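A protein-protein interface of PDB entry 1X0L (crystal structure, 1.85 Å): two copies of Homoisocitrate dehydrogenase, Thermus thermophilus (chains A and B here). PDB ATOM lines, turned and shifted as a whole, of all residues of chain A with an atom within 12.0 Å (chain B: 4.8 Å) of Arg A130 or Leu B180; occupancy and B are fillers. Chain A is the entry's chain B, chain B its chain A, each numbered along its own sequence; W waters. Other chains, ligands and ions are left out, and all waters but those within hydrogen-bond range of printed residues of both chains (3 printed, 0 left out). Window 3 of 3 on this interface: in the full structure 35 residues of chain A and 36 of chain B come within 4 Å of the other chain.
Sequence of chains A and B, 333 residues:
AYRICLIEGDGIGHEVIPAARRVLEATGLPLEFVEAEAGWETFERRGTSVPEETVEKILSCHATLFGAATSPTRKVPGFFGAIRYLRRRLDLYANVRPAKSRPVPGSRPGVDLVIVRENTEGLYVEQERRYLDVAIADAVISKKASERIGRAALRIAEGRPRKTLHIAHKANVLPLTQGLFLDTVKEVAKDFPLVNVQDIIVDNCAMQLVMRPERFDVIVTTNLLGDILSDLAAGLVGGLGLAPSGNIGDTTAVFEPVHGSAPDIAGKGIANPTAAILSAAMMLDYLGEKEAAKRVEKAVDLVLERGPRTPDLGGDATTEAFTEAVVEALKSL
Water W2 lies within hydrogen-bond range of the side-chain carboxylate (OD2) of Asp A133 and the backbone NH (N) of Lys B143. Water W3 bridges the backbone carbonyl oxygen of Leu B176 and the guanidinium group of Arg A130. Water W1 lies within hydrogen-bond range of the guanidinium group (NH2) of Arg A130, the side-chain amino group (NZ) of Lys B143 and the backbone carbonyl oxygen (O) of Leu A132.
The guanidinium group (NE) of Arg A130 lies within hydrogen-bond range of the backbone carbonyl oxygen (O) of Leu A132 (2.9 Å). The backbone carbonyl oxygen of Ser B142 lies within hydrogen-bond range of the side-chain hydroxyl of Ser B146 (2.9 Å). OD1 of Asp A138 is in salt-bridge range of NH2 of Arg A129 (3.2 Å). The backbone carbonyl oxygen (O) of Leu B180 is in hydrogen-bond range of the side-chain hydroxyl (OG1) of Thr B184 (2.7 Å). O of Arg A129 is in hydrogen-bond range of N of Ile A136, 2.7 Å away.
No position is printed for both chains. Of the 14 pairs that touch across the chains among the printed residues, none has its exchanged pair printed and touching as well.
Printed residues of chain A that touch a printed residue of chain B: Glu A128, Arg A129, Arg A130, Asp A133, Val A134, Ala A135, Ile A136 and Ala A137. Hydrophobic or aromatic side chains of chain B that line the printed part of chain A: Pro B175, Leu B176 and Leu B180. Among the printed residues, no Asp or Glu carboxylate lies within 4 Å of a Lys or Arg side-chain nitrogen of the other chain.
Arg A129 touches Leu B176 (N to CD1, 3.8 Å). Leu B180 touches Arg A130. Asp A133 touches Ser B142 (O to CA, 3.2 Å). O of Asp A133 touches CD1 of Leu B180, 3.8 Å away. Ile B141 touches Val A134 (O to C, 3.7 Å). O of Leu B176 touches CB of Ala A135, at 3.7 Å. CG2 of Thr B177 touches C of Ala A135, at 3.6 Å. Ile A136 touches Thr B177 (C to CG2, 3.5 Å). Thr B177 touches Ala A137 (CG2 to N, 3.5 Å).
Printed residues of chain B within 4 Å of Glu A128: Pro B175, Leu B176 and Thr B177. Arg A130 touches just one residue of chain B: Leu B180 (3.7 Å). Tyr A131 touches none of the printed residues of chain B. Of the printed residues of chain B, Asp A133 touches Ser B142 (3.2 Å), Lys B143 (3.1 Å) and Leu B180 (3.8 Å). Printed residues of chain B within 4 Å of Val A134: Ile B141 (3.7 Å). Of the printed residues of chain B, Ala A135 touches Ile B141, Leu B176 and Thr B177. Printed residues of chain B within 4 Å of Ala A137: Thr B177. Asp A138 touches none of the printed residues of chain B. Ser B142 touches just one residue of chain A: Asp A133. Lys B143 touches just one residue of chain A: Asp A133 (3.1 Å). No residue of chain A comes within 4 Å of Ser B146. Thr B177 touches just these residues of chain A: Glu A128, Ala A135, Ile A136 and Ala A137. No residue of chain A comes within 4 Å of Gly B179. Leu B180 touches two residues of chain A. No residue of chain A comes within 4 Å of Phe B181. Leu B182 touches none of the printed residues of chain A. No residue of chain A comes within 4 Å of Thr B184.
N of Thr B177 lies within hydrogen-bond range of OE2 of Glu A128. The backbone NH (N) of Leu B176 sits at hydrogen-bond distance from the side-chain carboxylate (OE1) of Glu A128. OE1 of Glu A128 sits close to N of Pro B175. The backbone carbonyl oxygen of Ile B141 is in hydrogen-bond range of the backbone NH of Ala A135. N of Lys B143 lies within hydrogen-bond range of O of Asp A133 (3.1 Å).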
ATOM      1  N   GLU A 126      17.847  20.654   7.133  1.00  0.00           N
ATOM      2  CA  GLU A 126      16.799  19.640   7.035  1.00  0.00           C
ATOM      3  C   GLU A 126      15.606  20.253   6.304  1.00  0.00           C
ATOM      4  O   GLU A 126      14.900  21.105   6.841  1.00  0.00           O
ATOM      5  CB  GLU A 126      16.396  19.169   8.431  1.00  0.00           C
ATOM      6  CG  GLU A 126      17.590  18.842   9.317  1.00  0.00           C
ATOM      7  CD  GLU A 126      17.194  18.178  10.620  1.00  0.00           C
ATOM      8  OE1 GLU A 126      17.024  16.940  10.630  1.00  0.00           O
ATOM      9  OE2 GLU A 126      17.047  18.898  11.632  1.00  0.00           O
ATOM     10  N   GLN A 127      15.389  19.794   5.076  1.00  0.00           N
ATOM     11  CA  GLN A 127      14.332  20.306   4.212  1.00  0.00           C
ATOM     12  C   GLN A 127      12.879  19.945   4.527  1.00  0.00           C
ATOM     13  O   GLN A 127      12.570  18.833   4.962  1.00  0.00           O
ATOM     14  CB  GLN A 127      14.625  19.889   2.770  1.00  0.00           C
ATOM     15  CG  GLN A 127      16.031  20.214   2.291  1.00  0.00           C
ATOM     16  CD  GLN A 127      16.303  21.701   2.210  1.00  0.00           C
ATOM     17  OE1 GLN A 127      15.514  22.458   1.646  1.00  0.00           O
ATOM     18  NE2 GLN A 127      17.433  22.126   2.761  1.00  0.00           N
ATOM     19  N   GLU A 128      12.000  20.914   4.291  1.00  0.00           N
ATOM     20  CA  GLU A 128      10.559  20.756   4.466  1.00  0.00           C
ATOM     21  C   GLU A 128       9.986  20.846   3.066  1.00  0.00           C
ATOM     22  O   GLU A 128      10.516  21.575   2.227  1.00  0.00           O
ATOM     23  CB  GLU A 128       9.957  21.892   5.288  1.00  0.00           C
ATOM     24  CG  GLU A 128       9.887  21.651   6.761  1.00  0.00           C
ATOM     25  CD  GLU A 128       8.825  22.511   7.413  1.00  0.00           C
ATOM     26  OE1 GLU A 128       8.918  23.754   7.319  1.00  0.00           O
ATOM     27  OE2 GLU A 128       7.890  21.937   8.009  1.00  0.00           O
ATOM     28  N   ARG A 129       8.899  20.122   2.818  1.00  0.00           N
ATOM     29  CA  ARG A 129       8.277  20.120   1.504  1.00  0.00           C
ATOM     30  C   ARG A 129       6.772  19.923   1.641  1.00  0.00           C
ATOM     31  O   ARG A 129       6.315  19.194   2.520  1.00  0.00           O
ATOM     32  CB  ARG A 129       8.834  18.969   0.661  1.00  0.00           C
ATOM     33  CG  ARG A 129      10.346  18.853   0.648  1.00  0.00           C
ATOM     34  CD  ARG A 129      10.783  17.450   0.259  1.00  0.00           C
ATOM     35  NE  ARG A 129      10.407  16.468   1.273  1.00  0.00           N
ATOM     36  CZ  ARG A 129      10.629  15.162   1.167  1.00  0.00           C
ATOM     37  NH1 ARG A 129      11.226  14.673   0.091  1.00  0.00           N
ATOM     38  NH2 ARG A 129      10.245  14.342   2.135  1.00  0.00           N
ATOM     39  N   ARG A 130       6.003  20.574   0.779  1.00  0.00           N
ATOM     40  CA  ARG A 130       4.561  20.388   0.802  1.00  0.00           C
ATOM     41  C   ARG A 130       4.056  20.088  -0.600  1.00  0.00           C
ATOM     42  O   ARG A 130       4.421  20.762  -1.566  1.00  0.00           O
ATOM     43  CB  ARG A 130       3.834  21.608   1.366  1.00  0.00           C
ATOM     44  CG  ARG A 130       2.323  21.382   1.411  1.00  0.00           C
ATOM     45  CD  ARG A 130       1.593  22.388   2.266  1.00  0.00           C
ATOM     46  NE  ARG A 130       0.146  22.255   2.110  1.00  0.00           N
ATOM     47  CZ  ARG A 130      -0.741  23.074   2.662  1.00  0.00           C
ATOM     48  NH1 ARG A 130      -0.330  24.083   3.417  1.00  0.00           N
ATOM     49  NH2 ARG A 130      -2.035  22.903   2.436  1.00  0.00           N
ATOM     50  N   TYR A 131       3.237  19.046  -0.695  1.00  0.00           N
ATOM     51  CA  TYR A 131       2.644  18.600  -1.946  1.00  0.00           C
ATOM     52  C   TYR A 131       1.146  18.513  -1.684  1.00  0.00           C
ATOM     53  O   TYR A 131       0.681  17.604  -0.994  1.00  0.00           O
ATOM     54  CB  TYR A 131       3.192  17.220  -2.325  1.00  0.00           C
ATOM     55  CG  TYR A 131       4.692  17.202  -2.560  1.00  0.00           C
ATOM     56  CD1 TYR A 131       5.529  16.351  -1.833  1.00  0.00           C
ATOM     57  CD2 TYR A 131       5.272  18.037  -3.514  1.00  0.00           C
ATOM     58  CE1 TYR A 131       6.919  16.338  -2.057  1.00  0.00           C
ATOM     59  CE2 TYR A 131       6.649  18.030  -3.742  1.00  0.00           C
ATOM     60  CZ  TYR A 131       7.464  17.183  -3.016  1.00  0.00           C
ATOM     61  OH  TYR A 131       8.823  17.183  -3.268  1.00  0.00           O
ATOM     62  N   LEU A 132       0.398  19.465  -2.229  1.00  0.00           N
ATOM     63  CA  LEU A 132      -1.047  19.512  -2.034  1.00  0.00           C
ATOM     64  C   LEU A 132      -1.383  19.563  -0.539  1.00  0.00           C
ATOM     65  O   LEU A 132      -0.947  20.472   0.161  1.00  0.00           O
ATOM     66  CB  LEU A 132      -1.716  18.296  -2.680  1.00  0.00           C
ATOM     67  CG  LEU A 132      -1.519  18.149  -4.193  1.00  0.00           C
ATOM     68  CD1 LEU A 132      -2.374  17.000  -4.705  1.00  0.00           C
ATOM     69  CD2 LEU A 132      -1.899  19.442  -4.891  1.00  0.00           C
ATOM     70  N   ASP A 133      -2.130  18.572  -0.058  1.00  0.00           N
ATOM     71  CA  ASP A 133      -2.564  18.507   1.342  1.00  0.00           C
ATOM     72  C   ASP A 133      -1.600  17.787   2.287  1.00  0.00           C
ATOM     73  O   ASP A 133      -1.916  17.579   3.464  1.00  0.00           O
ATOM     74  CB  ASP A 133      -3.932  17.818   1.407  1.00  0.00           C
ATOM     75  CG  ASP A 133      -3.907  16.406   0.810  1.00  0.00           C
ATOM     76  OD1 ASP A 133      -3.304  16.225  -0.269  1.00  0.00           O
ATOM     77  OD2 ASP A 133      -4.493  15.475   1.406  1.00  0.00           O
ATOM     78  N   VAL A 134      -0.429  17.415   1.779  1.00  0.00           N
ATOM     79  CA  VAL A 134       0.553  16.692   2.578  1.00  0.00           C
ATOM     80  C   VAL A 134       1.875  17.442   2.714  1.00  0.00           C
ATOM     81  O   VAL A 134       2.467  17.853   1.718  1.00  0.00           O
ATOM     82  CB  VAL A 134       0.839  15.304   1.943  1.00  0.00           C
ATOM     83  CG1 VAL A 134       1.824  14.522   2.794  1.00  0.00           C
ATOM     84  CG2 VAL A 134      -0.457  14.539   1.777  1.00  0.00           C
ATOM     85  N   ALA A 135       2.332  17.618   3.950  1.00  0.00           N
ATOM     86  CA  ALA A 135       3.602  18.297   4.203  1.00  0.00           C
ATOM     87  C   ALA A 135       4.553  17.296   4.849  1.00  0.00           C
ATOM     88  O   ALA A 135       4.154  16.514   5.711  1.00  0.00           O
ATOM     89  CB  ALA A 135       3.398  19.497   5.118  1.00  0.00           C
ATOM     90  N   ILE A 136       5.816  17.334   4.435  1.00  0.00           N
ATOM     91  CA  ILE A 136       6.816  16.408   4.945  1.00  0.00           C
ATOM     92  C   ILE A 136       8.075  17.135   5.394  1.00  0.00           C
ATOM     93  O   ILE A 136       8.597  17.984   4.671  1.00  0.00           O
ATOM     94  CB  ILE A 136       7.217  15.393   3.856  1.00  0.00           C
ATOM     95  CG1 ILE A 136       5.972  14.693   3.311  1.00  0.00           C
ATOM     96  CG2 ILE A 136       8.189  14.369   4.431  1.00  0.00           C
ATOM     97  CD1 ILE A 136       6.232  13.848   2.079  1.00  0.00           C
ATOM     98  N   ALA A 137       8.556  16.791   6.585  1.00  0.00           N
ATOM     99  CA  ALA A 137       9.771  17.388   7.134  1.00  0.00           C
ATOM    100  C   ALA A 137      10.810  16.289   7.328  1.00  0.00           C
ATOM    101  O   ALA A 137      10.518  15.255   7.933  1.00  0.00           O
ATOM    102  CB  ALA A 137       9.475  18.056   8.462  1.00  0.00           C
ATOM    103  N   ASP A 138      12.018  16.512   6.817  1.00  0.00           N
ATOM    104  CA  ASP A 138      13.086  15.524   6.948  1.00  0.00           C
ATOM    105  C   ASP A 138      13.813  15.620   8.281  1.00  0.00           C
ATOM    106  O   ASP A 138      14.191  16.707   8.711  1.00  0.00           O
ATOM    107  CB  ASP A 138      14.141  15.696   5.843  1.00  0.00           C
ATOM    108  CG  ASP A 138      13.647  15.276   4.475  1.00  0.00           C
ATOM    109  OD1 ASP A 138      12.531  14.727   4.378  1.00  0.00           O
ATOM    110  OD2 ASP A 138      14.392  15.496   3.494  1.00  0.00           O
ATOM    111  N   ILE B 141       2.597  15.581   8.029  1.00  0.00           N
ATOM    112  CA  ILE B 141       1.417  16.284   8.509  1.00  0.00           C
ATOM    113  C   ILE B 141       0.501  16.497   7.308  1.00  0.00           C
ATOM    114  O   ILE B 141       0.952  16.928   6.241  1.00  0.00           O
ATOM    115  CB  ILE B 141       1.780  17.658   9.104  1.00  0.00           C
ATOM    116  CG1 ILE B 141       2.635  17.469  10.364  1.00  0.00           C
ATOM    117  CG2 ILE B 141       0.509  18.458   9.398  1.00  0.00           C
ATOM    118  CD1 ILE B 141       1.927  16.745  11.508  1.00  0.00           C
ATOM    119  N   SER B 142      -0.775  16.177   7.467  1.00  0.00           N
ATOM    120  CA  SER B 142      -1.722  16.369   6.376  1.00  0.00           C
ATOM    121  C   SER B 142      -2.910  17.162   6.892  1.00  0.00           C
ATOM    122  O   SER B 142      -3.193  17.167   8.094  1.00  0.00           O
ATOM    123  CB  SER B 142      -2.201  15.021   5.824  1.00  0.00           C
ATOM    124  OG  SER B 142      -3.051  14.347   6.740  1.00  0.00           O
ATOM    125  N   LYS B 143      -3.603  17.845   5.992  1.00  0.00           N
ATOM    126  CA  LYS B 143      -4.760  18.620   6.412  1.00  0.00           C
ATOM    127  C   LYS B 143      -5.808  17.684   7.007  1.00  0.00           C
ATOM    128  O   LYS B 143      -6.371  17.971   8.062  1.00  0.00           O
ATOM    129  CB  LYS B 143      -5.350  19.397   5.230  1.00  0.00           C
ATOM    130  CG  LYS B 143      -6.558  20.254   5.600  1.00  0.00           C
ATOM    131  CD  LYS B 143      -7.075  21.062   4.411  1.00  0.00           C
ATOM    132  CE  LYS B 143      -6.054  22.095   3.947  1.00  0.00           C
ATOM    133  NZ  LYS B 143      -6.582  22.981   2.870  1.00  0.00           N
ATOM    134  N   SER B 146      -4.842  16.505  10.479  1.00  0.00           N
ATOM    135  CA  SER B 146      -4.891  17.621  11.415  1.00  0.00           C
ATOM    136  C   SER B 146      -6.331  18.036  11.725  1.00  0.00           C
ATOM    137  O   SER B 146      -6.653  18.370  12.865  1.00  0.00           O
ATOM    138  CB  SER B 146      -4.103  18.815  10.859  1.00  0.00           C
ATOM    139  OG  SER B 146      -2.745  18.461  10.648  1.00  0.00           O
ATOM    140  N   PRO B 175       7.632  25.670   9.599  1.00  0.00           N
ATOM    141  CA  PRO B 175       6.477  26.381   9.049  1.00  0.00           C
ATOM    142  C   PRO B 175       5.554  25.606   8.121  1.00  0.00           C
ATOM    143  O   PRO B 175       4.347  25.812   8.157  1.00  0.00           O
ATOM    144  CB  PRO B 175       7.113  27.589   8.363  1.00  0.00           C
ATOM    145  CG  PRO B 175       8.423  27.050   7.905  1.00  0.00           C
ATOM    146  CD  PRO B 175       8.887  26.272   9.114  1.00  0.00           C
ATOM    147  N   LEU B 176       6.103  24.724   7.290  1.00  0.00           N
ATOM    148  CA  LEU B 176       5.261  23.962   6.369  1.00  0.00           C
ATOM    149  C   LEU B 176       4.486  22.836   7.048  1.00  0.00           C
ATOM    150  O   LEU B 176       3.265  22.751   6.908  1.00  0.00           O
ATOM    151  CB  LEU B 176       6.094  23.383   5.219  1.00  0.00           C
ATOM    152  CG  LEU B 176       6.750  24.377   4.255  1.00  0.00           C
ATOM    153  CD1 LEU B 176       7.336  23.616   3.077  1.00  0.00           C
ATOM    154  CD2 LEU B 176       5.727  25.387   3.759  1.00  0.00           C
ATOM    155  N   THR B 177       5.181  21.971   7.783  1.00  0.00           N
ATOM    156  CA  THR B 177       4.501  20.862   8.452  1.00  0.00           C
ATOM    157  C   THR B 177       3.760  21.301   9.708  1.00  0.00           C
ATOM    158  O   THR B 177       2.545  21.125   9.810  1.00  0.00           O
ATOM    159  CB  THR B 177       5.479  19.725   8.823  1.00  0.00           C
ATOM    160  OG1 THR B 177       6.530  20.239   9.649  1.00  0.00           O
ATOM    161  CG2 THR B 177       6.069  19.098   7.562  1.00  0.00           C
ATOM    162  N   GLN B 178       4.484  21.875  10.665  1.00  0.00           N
ATOM    163  CA  GLN B 178       3.859  22.327  11.902  1.00  0.00           C
ATOM    164  C   GLN B 178       2.889  23.477  11.640  1.00  0.00           C
ATOM    165  O   GLN B 178       1.905  23.639  12.358  1.00  0.00           O
ATOM    166  CB  GLN B 178       4.927  22.748  12.918  1.00  0.00           C
ATOM    167  CG  GLN B 178       5.691  21.579  13.561  1.00  0.00           C
ATOM    168  CD  GLN B 178       4.831  20.769  14.531  1.00  0.00           C
ATOM    169  OE1 GLN B 178       4.181  21.331  15.412  1.00  0.00           O
ATOM    170  NE2 GLN B 178       4.833  19.447  14.376  1.00  0.00           N
ATOM    171  N   GLY B 179       3.162  24.270  10.607  1.00  0.00           N
ATOM    172  CA  GLY B 179       2.274  25.374  10.285  1.00  0.00           C
ATOM    173  C   GLY B 179       0.950  24.862   9.746  1.00  0.00           C
ATOM    174  O   GLY B 179      -0.111  25.414  10.050  1.00  0.00           O
ATOM    175  N   LEU B 180       1.010  23.805   8.938  1.00  0.00           N
ATOM    176  CA  LEU B 180      -0.195  23.208   8.366  1.00  0.00           C
ATOM    177  C   LEU B 180      -1.043  22.686   9.525  1.00  0.00           C
ATOM    178  O   LEU B 180      -2.260  22.869   9.561  1.00  0.00           O
ATOM    179  CB  LEU B 180       0.168  22.040   7.444  1.00  0.00           C
ATOM    180  CG  LEU B 180      -0.751  21.711   6.262  1.00  0.00           C
ATOM    181  CD1 LEU B 180      -0.657  20.223   5.962  1.00  0.00           C
ATOM    182  CD2 LEU B 180      -2.189  22.097   6.554  1.00  0.00           C
ATOM    183  N   PHE B 181      -0.386  22.025  10.468  1.00  0.00           N
ATOM    184  CA  PHE B 181      -1.066  21.485  11.642  1.00  0.00           C
ATOM    185  C   PHE B 181      -1.763  22.600  12.421  1.00  0.00           C
ATOM    186  O   PHE B 181      -2.971  22.539  12.671  1.00  0.00           O
ATOM    187  CB  PHE B 181      -0.051  20.787  12.553  1.00  0.00           C
ATOM    188  CG  PHE B 181      -0.610  20.383  13.892  1.00  0.00           C
ATOM    189  CD1 PHE B 181      -1.548  19.360  13.992  1.00  0.00           C
ATOM    190  CD2 PHE B 181      -0.204  21.038  15.052  1.00  0.00           C
ATOM    191  CE1 PHE B 181      -2.075  18.994  15.238  1.00  0.00           C
ATOM    192  CE2 PHE B 181      -0.724  20.680  16.297  1.00  0.00           C
ATOM    193  CZ  PHE B 181      -1.664  19.652  16.386  1.00  0.00           C
ATOM    194  N   LEU B 182      -0.991  23.618  12.786  1.00  0.00           N
ATOM    195  CA  LEU B 182      -1.489  24.753  13.563  1.00  0.00           C
ATOM    196  C   LEU B 182      -2.663  25.445  12.880  1.00  0.00           C
ATOM    197  O   LEU B 182      -3.734  25.603  13.473  1.00  0.00           O
ATOM    198  CB  LEU B 182      -0.364  25.771  13.775  1.00  0.00           C
ATOM    199  CG  LEU B 182      -0.237  26.597  15.061  1.00  0.00           C
ATOM    200  CD1 LEU B 182       0.426  27.922  14.713  1.00  0.00           C
ATOM    201  CD2 LEU B 182      -1.585  26.833  15.722  1.00  0.00           C
ATOM    202  N   ASP B 183      -2.454  25.857  11.634  1.00  0.00           N
ATOM    203  CA  ASP B 183      -3.496  26.553  10.884  1.00  0.00           C
ATOM    204  C   ASP B 183      -4.770  25.737  10.740  1.00  0.00           C
ATOM    205  O   ASP B 183      -5.875  26.275  10.855  1.00  0.00           O
ATOM    206  CB  ASP B 183      -2.997  26.950   9.488  1.00  0.00           C
ATOM    207  CG  ASP B 183      -1.840  27.933   9.529  1.00  0.00           C
ATOM    208  OD1 ASP B 183      -1.662  28.614  10.558  1.00  0.00           O
ATOM    209  OD2 ASP B 183      -1.117  28.033   8.517  1.00  0.00           O
ATOM    210  N   THR B 184      -4.625  24.439  10.489  1.00  0.00           N
ATOM    211  CA  THR B 184      -5.789  23.584  10.318  1.00  0.00           C
ATOM    212  C   THR B 184      -6.605  23.453  11.597  1.00  0.00           C
ATOM    213  O   THR B 184      -7.835  23.563  11.573  1.00  0.00           O
ATOM    214  CB  THR B 184      -5.375  22.193   9.811  1.00  0.00           C
ATOM    215  OG1 THR B 184      -4.682  22.339   8.566  1.00  0.00           O
ATOM    216  CG2 THR B 184      -6.598  21.316   9.588  1.00  0.00           C
HETATM  217  O   HOH W   1      -4.259  21.187   1.015  1.00  0.00           O
HETATM  218  O   HOH W   2      -5.429  15.983   3.680  1.00  0.00           O
HETATM  219  O   HOH W   3       2.045  24.315   4.982  1.00  0.00           O
